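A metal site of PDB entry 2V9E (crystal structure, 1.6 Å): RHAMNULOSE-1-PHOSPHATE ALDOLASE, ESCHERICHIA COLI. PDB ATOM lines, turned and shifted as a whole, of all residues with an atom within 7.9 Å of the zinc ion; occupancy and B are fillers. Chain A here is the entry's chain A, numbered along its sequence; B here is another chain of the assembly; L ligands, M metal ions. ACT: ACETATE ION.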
ATOM      1  N   TRP A  25      15.670  11.874  -9.640  1.00  0.00           N
ATOM      2  CA  TRP A  25      16.080  11.224 -10.897  1.00  0.00           C
ATOM      3  C   TRP A  25      17.123  10.140 -10.709  1.00  0.00           C
ATOM      4  O   TRP A  25      17.513   9.479 -11.684  1.00  0.00           O
ATOM      5  CB  TRP A  25      16.690  12.260 -11.850  1.00  0.00           C
ATOM      6  CG  TRP A  25      15.770  13.354 -12.272  1.00  0.00           C
ATOM      7  CD1 TRP A  25      14.393  13.395 -12.189  1.00  0.00           C
ATOM      8  CD2 TRP A  25      16.165  14.561 -12.926  1.00  0.00           C
ATOM      9  NE1 TRP A  25      13.918  14.570 -12.713  1.00  0.00           N
ATOM     10  CE2 TRP A  25      14.987  15.301 -13.187  1.00  0.00           C
ATOM     11  CE3 TRP A  25      17.407  15.105 -13.290  1.00  0.00           C
ATOM     12  CZ2 TRP A  25      15.013  16.566 -13.801  1.00  0.00           C
ATOM     13  CZ3 TRP A  25      17.438  16.360 -13.904  1.00  0.00           C
ATOM     14  CH2 TRP A  25      16.244  17.070 -14.158  1.00  0.00           C
ATOM     15  N   ASP A  26      17.636   9.972  -9.489  1.00  0.00           N
ATOM     16  CA  ASP A  26      18.829   9.146  -9.314  1.00  0.00           C
ATOM     17  C   ASP A  26      18.828   8.353  -8.007  1.00  0.00           C
ATOM     18  O   ASP A  26      19.740   8.490  -7.164  1.00  0.00           O
ATOM     19  CB  ASP A  26      20.103   9.985  -9.499  1.00  0.00           C
ATOM     20  CG  ASP A  26      20.206  10.546 -10.902  1.00  0.00           C
ATOM     21  OD1 ASP A  26      19.888  11.716 -11.077  1.00  0.00           O
ATOM     22  OD2 ASP A  26      20.569   9.783 -11.837  1.00  0.00           O
ATOM     23  N   GLU A  27      17.806   7.519  -7.876  1.00  0.00           N
ATOM     24  CA  GLU A  27      17.740   6.500  -6.830  1.00  0.00           C
ATOM     25  C   GLU A  27      18.981   5.601  -6.835  1.00  0.00           C
ATOM     26  O   GLU A  27      19.544   5.322  -7.896  1.00  0.00           O
ATOM     27  CB  GLU A  27      16.475   5.651  -7.008  1.00  0.00           C
ATOM     28  CG  GLU A  27      16.497   4.654  -8.210  1.00  0.00           C
ATOM     29  CD  GLU A  27      16.184   5.258  -9.592  1.00  0.00           C
ATOM     30  OE1 GLU A  27      16.183   4.504 -10.628  1.00  0.00           O
ATOM     31  OE2 GLU A  27      15.939   6.495  -9.638  1.00  0.00           O
ATOM     32  N   ASN A  29      22.200   3.798  -7.286  1.00  0.00           N
ATOM     33  CA  ASN A  29      23.315   4.187  -8.164  1.00  0.00           C
ATOM     34  C   ASN A  29      22.842   4.514  -9.580  1.00  0.00           C
ATOM     35  O   ASN A  29      23.649   4.502 -10.527  1.00  0.00           O
ATOM     36  CB  ASN A  29      24.381   3.082  -8.217  1.00  0.00           C
ATOM     37  CG  ASN A  29      23.840   1.804  -8.811  1.00  0.00           C
ATOM     38  OD1 ASN A  29      22.739   1.379  -8.454  1.00  0.00           O
ATOM     39  ND2 ASN A  29      24.589   1.177  -9.713  1.00  0.00           N
ATOM     40  N   GLY A  30      21.554   4.829  -9.718  1.00  0.00           N
ATOM     41  CA  GLY A  30      20.895   5.019 -11.015  1.00  0.00           C
ATOM     42  C   GLY A  30      21.144   6.353 -11.674  1.00  0.00           C
ATOM     43  O   GLY A  30      20.264   7.236 -11.690  1.00  0.00           O
ATOM     44  N   GLY A  31      22.308   6.472 -12.298  1.00  0.00           N
ATOM     45  CA  GLY A  31      22.756   7.719 -12.924  1.00  0.00           C
ATOM     46  C   GLY A  31      24.262   7.722 -13.052  1.00  0.00           C
ATOM     47  O   GLY A  31      24.979   7.043 -12.307  1.00  0.00           O
ATOM     48  N   ASN A  32      24.758   8.484 -14.011  1.00  0.00           N
ATOM     49  CA  ASN A  32      26.201   8.667 -14.152  1.00  0.00           C
ATOM     50  C   ASN A  32      26.481   9.932 -14.952  1.00  0.00           C
ATOM     51  O   ASN A  32      25.667  10.365 -15.768  1.00  0.00           O
ATOM     52  CB  ASN A  32      26.920   7.437 -14.755  1.00  0.00           C
ATOM     53  CG  ASN A  32      25.992   6.537 -15.532  1.00  0.00           C
ATOM     54  OD1 ASN A  32      25.658   6.823 -16.678  1.00  0.00           O
ATOM     55  ND2 ASN A  32      25.584   5.435 -14.905  1.00  0.00           N
ATOM     56  N   SER A 116      29.939   1.974 -14.649  1.00  0.00           N
ATOM     57  CA  SER A 116      29.754   0.847 -15.555  1.00  0.00           C
ATOM     58  C   SER A 116      29.268   1.259 -16.944  1.00  0.00           C
ATOM     59  O   SER A 116      29.315   0.454 -17.894  1.00  0.00           O
ATOM     60  CB  SER A 116      28.751  -0.161 -14.961  1.00  0.00           C
ATOM     61  OG  SER A 116      27.502   0.460 -14.750  1.00  0.00           O
ATOM     62  N   GLU A 117      28.797   2.509 -17.080  1.00  0.00           N
ATOM     63  CA  GLU A 117      28.325   3.022 -18.377  1.00  0.00           C
ATOM     64  C   GLU A 117      29.399   3.848 -19.082  1.00  0.00           C
ATOM     65  O   GLU A 117      29.104   4.638 -19.993  1.00  0.00           O
ATOM     66  CB  GLU A 117      27.047   3.851 -18.210  1.00  0.00           C
ATOM     67  CG  GLU A 117      25.849   3.032 -17.715  1.00  0.00           C
ATOM     68  CD  GLU A 117      25.336   2.000 -18.726  1.00  0.00           C
ATOM     69  OE1 GLU A 117      25.867   1.881 -19.846  1.00  0.00           O
ATOM     70  OE2 GLU A 117      24.393   1.285 -18.365  1.00  0.00           O
ATOM     71  N   HIS A 141      23.655  10.955 -17.609  1.00  0.00           N
ATOM     72  CA  HIS A 141      22.607   9.943 -17.645  1.00  0.00           C
ATOM     73  C   HIS A 141      21.870  10.007 -16.326  1.00  0.00           C
ATOM     74  O   HIS A 141      22.478   9.996 -15.248  1.00  0.00           O
ATOM     75  CB  HIS A 141      23.184   8.543 -17.842  1.00  0.00           C
ATOM     76  CG  HIS A 141      22.215   7.428 -17.552  1.00  0.00           C
ATOM     77  ND1 HIS A 141      21.009   7.291 -18.209  1.00  0.00           N
ATOM     78  CD2 HIS A 141      22.301   6.391 -16.684  1.00  0.00           C
ATOM     79  CE1 HIS A 141      20.385   6.217 -17.734  1.00  0.00           C
ATOM     80  NE2 HIS A 141      21.152   5.650 -16.826  1.00  0.00           N
ATOM     81  N   CYS A 142      20.557  10.009 -16.358  1.00  0.00           N
ATOM     82  CA  CYS A 142      19.824   9.814 -15.092  1.00  0.00           C
ATOM     83  C   CYS A 142      18.525   9.087 -15.447  1.00  0.00           C
ATOM     84  O   CYS A 142      18.231   8.772 -16.619  1.00  0.00           O
ATOM     85  CB  CYS A 142      19.487  11.167 -14.403  1.00  0.00           C
ATOM     86  SG  CYS A 142      18.474  12.296 -15.532  1.00  0.00           S
ATOM     87  N   HIS A 143      17.759   8.887 -14.414  1.00  0.00           N
ATOM     88  CA  HIS A 143      16.512   8.143 -14.471  1.00  0.00           C
ATOM     89  C   HIS A 143      15.354   9.114 -14.317  1.00  0.00           C
ATOM     90  O   HIS A 143      14.647   9.125 -13.302  1.00  0.00           O
ATOM     91  CB  HIS A 143      16.526   7.030 -13.428  1.00  0.00           C
ATOM     92  CG  HIS A 143      17.575   5.987 -13.675  1.00  0.00           C
ATOM     93  ND1 HIS A 143      17.689   4.848 -12.900  1.00  0.00           N
ATOM     94  CD2 HIS A 143      18.562   5.900 -14.608  1.00  0.00           C
ATOM     95  CE1 HIS A 143      18.679   4.105 -13.352  1.00  0.00           C
ATOM     96  NE2 HIS A 143      19.227   4.709 -14.393  1.00  0.00           N
ATOM     97  N   ILE A 148      10.783   8.457 -18.364  1.00  0.00           N
ATOM     98  CA  ILE A 148      10.668   6.991 -18.242  1.00  0.00           C
ATOM     99  C   ILE A 148       9.210   6.551 -18.389  1.00  0.00           C
ATOM    100  O   ILE A 148       8.896   5.665 -19.188  1.00  0.00           O
ATOM    101  CB  ILE A 148      11.279   6.450 -16.909  1.00  0.00           C
ATOM    102  CG1 ILE A 148      12.796   6.670 -16.844  1.00  0.00           C
ATOM    103  CG2 ILE A 148      10.964   4.949 -16.745  1.00  0.00           C
ATOM    104  CD1 ILE A 148      13.309   6.577 -15.438  1.00  0.00           C
ATOM    105  N   PRO A 188      21.692  -2.934 -20.227  1.00  0.00           N
ATOM    106  CA  PRO A 188      22.607  -1.836 -19.961  1.00  0.00           C
ATOM    107  C   PRO A 188      24.010  -2.282 -19.543  1.00  0.00           C
ATOM    108  O   PRO A 188      24.239  -3.461 -19.256  1.00  0.00           O
ATOM    109  CB  PRO A 188      21.906  -1.071 -18.819  1.00  0.00           C
ATOM    110  CG  PRO A 188      21.209  -2.139 -18.077  1.00  0.00           C
ATOM    111  CD  PRO A 188      20.742  -3.148 -19.114  1.00  0.00           C
ATOM    112  N   GLY A 189      24.952  -1.339 -19.551  1.00  0.00           N
ATOM    113  CA  GLY A 189      26.319  -1.566 -19.084  1.00  0.00           C
ATOM    114  C   GLY A 189      27.177  -2.332 -20.067  1.00  0.00           C
ATOM    115  O   GLY A 189      28.205  -2.897 -19.694  1.00  0.00           O
ATOM    116  N   TRP A 209      16.586   5.765 -23.317  1.00  0.00           N
ATOM    117  CA  TRP A 209      16.669   4.329 -23.061  1.00  0.00           C
ATOM    118  C   TRP A 209      15.313   3.914 -22.505  1.00  0.00           C
ATOM    119  O   TRP A 209      15.017   4.203 -21.336  1.00  0.00           O
ATOM    120  CB  TRP A 209      17.775   4.068 -22.033  1.00  0.00           C
ATOM    121  CG  TRP A 209      19.169   4.165 -22.567  1.00  0.00           C
ATOM    122  CD1 TRP A 209      19.577   4.632 -23.796  1.00  0.00           C
ATOM    123  CD2 TRP A 209      20.355   3.774 -21.870  1.00  0.00           C
ATOM    124  NE1 TRP A 209      20.954   4.546 -23.902  1.00  0.00           N
ATOM    125  CE2 TRP A 209      21.460   4.010 -22.746  1.00  0.00           C
ATOM    126  CE3 TRP A 209      20.606   3.234 -20.601  1.00  0.00           C
ATOM    127  CZ2 TRP A 209      22.782   3.734 -22.366  1.00  0.00           C
ATOM    128  CZ3 TRP A 209      21.930   2.948 -20.234  1.00  0.00           C
ATOM    129  CH2 TRP A 209      23.004   3.189 -21.127  1.00  0.00           C
ATOM    130  N   HIS A 212      14.077   2.903 -18.761  1.00  0.00           N
ATOM    131  CA  HIS A 212      15.343   3.062 -18.053  1.00  0.00           C
ATOM    132  C   HIS A 212      15.685   4.518 -17.751  1.00  0.00           C
ATOM    133  O   HIS A 212      15.783   4.921 -16.599  1.00  0.00           O
ATOM    134  CB  HIS A 212      16.481   2.328 -18.795  1.00  0.00           C
ATOM    135  CG  HIS A 212      17.799   2.368 -18.087  1.00  0.00           C
ATOM    136  ND1 HIS A 212      18.793   1.433 -18.303  1.00  0.00           N
ATOM    137  CD2 HIS A 212      18.286   3.214 -17.140  1.00  0.00           C
ATOM    138  CE1 HIS A 212      19.843   1.719 -17.543  1.00  0.00           C
ATOM    139  NE2 HIS A 212      19.550   2.792 -16.831  1.00  0.00           N
ATOM    140  N   GLY A 213      15.889   5.338 -18.781  1.00  0.00           N
ATOM    141  CA  GLY A 213      16.244   6.720 -18.515  1.00  0.00           C
ATOM    142  C   GLY A 213      16.688   7.466 -19.745  1.00  0.00           C
ATOM    143  O   GLY A 213      16.273   7.147 -20.858  1.00  0.00           O
ATOM    144  N   VAL A 214      17.523   8.476 -19.524  1.00  0.00           N
ATOM    145  CA  VAL A 214      17.876   9.418 -20.591  1.00  0.00           C
ATOM    146  C   VAL A 214      19.374   9.728 -20.549  1.00  0.00           C
ATOM    147  O   VAL A 214      19.988   9.686 -19.474  1.00  0.00           O
ATOM    148  CB  VAL A 214      17.005  10.716 -20.506  1.00  0.00           C
ATOM    149  CG1 VAL A 214      17.344  11.543 -19.247  1.00  0.00           C
ATOM    150  CG2 VAL A 214      17.109  11.565 -21.775  1.00  0.00           C
ATOM    151  N   PHE A 215      19.956   9.995 -21.717  1.00  0.00           N
ATOM    152  CA  PHE A 215      21.301  10.534 -21.846  1.00  0.00           C
ATOM    153  C   PHE A 215      21.201  11.912 -22.503  1.00  0.00           C
ATOM    154  O   PHE A 215      20.450  12.101 -23.464  1.00  0.00           O
ATOM    155  CB  PHE A 215      22.177   9.635 -22.734  1.00  0.00           C
ATOM    156  CG  PHE A 215      22.870   8.560 -21.988  1.00  0.00           C
ATOM    157  CD1 PHE A 215      22.151   7.483 -21.474  1.00  0.00           C
ATOM    158  CD2 PHE A 215      24.246   8.634 -21.746  1.00  0.00           C
ATOM    159  CE1 PHE A 215      22.814   6.470 -20.753  1.00  0.00           C
ATOM    160  CE2 PHE A 215      24.906   7.619 -21.039  1.00  0.00           C
ATOM    161  CZ  PHE A 215      24.193   6.544 -20.533  1.00  0.00           C
ATOM    162  N   THR B 170      14.417  -0.550 -15.336  1.00  0.00           N
ATOM    163  CA  THR B 170      15.321  -1.621 -15.792  1.00  0.00           C
ATOM    164  C   THR B 170      16.158  -2.256 -14.684  1.00  0.00           C
ATOM    165  O   THR B 170      16.309  -3.474 -14.653  1.00  0.00           O
ATOM    166  CB  THR B 170      16.193  -1.123 -16.959  1.00  0.00           C
ATOM    167  OG1 THR B 170      15.379  -0.975 -18.120  1.00  0.00           O
ATOM    168  CG2 THR B 170      17.339  -2.117 -17.267  1.00  0.00           C
ATOM    169  N   GLU B 171      16.687  -1.446 -13.769  1.00  0.00           N
ATOM    170  CA  GLU B 171      17.608  -1.985 -12.777  1.00  0.00           C
ATOM    171  C   GLU B 171      16.930  -2.791 -11.662  1.00  0.00           C
ATOM    172  O   GLU B 171      17.623  -3.400 -10.843  1.00  0.00           O
ATOM    173  CB  GLU B 171      18.434  -0.852 -12.187  1.00  0.00           C
ATOM    174  CG  GLU B 171      17.660   0.013 -11.226  1.00  0.00           C
ATOM    175  CD  GLU B 171      16.915   1.214 -11.827  1.00  0.00           C
ATOM    176  OE1 GLU B 171      16.460   1.994 -10.964  1.00  0.00           O
ATOM    177  OE2 GLU B 171      16.769   1.379 -13.085  1.00  0.00           O
HETATM  178  C   ACT L   1      22.604   2.872 -14.136  1.00  0.00           C
HETATM  179  O   ACT L   1      22.649   3.693 -15.056  1.00  0.00           O
HETATM  180  OXT ACT L   1      21.504   2.461 -13.715  1.00  0.00           O
HETATM  181  CH3 ACT L   1      23.877   2.399 -13.516  1.00  0.00           C
HETATM  182 ZN    ZN M   1      20.721   3.983 -15.638  1.00  0.00          ZN
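The backbone NH (N) of His 141 lies within hydrogen-bond range of the backbone carbonyl oxygen (O) of Asn 32 (2.8 Å).
N of His 143 lies within hydrogen-bond range of O of Trp 25 (2.8 Å).
O of Val 214 sits at hydrogen-bond distance from ND1 of His 141, 2.9 Å away.
ND1 of His 143 lies within hydrogen-bond range of OE1 of Glu 27.
The nearest printed residue that does not touch the zinc ion is Gly 31 (4.5 Å).
The zinc ion is bound by O of the ligand, NE2 of His 212, NE2 of His 143, NE2 of His 141 and OXT of the ligand.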
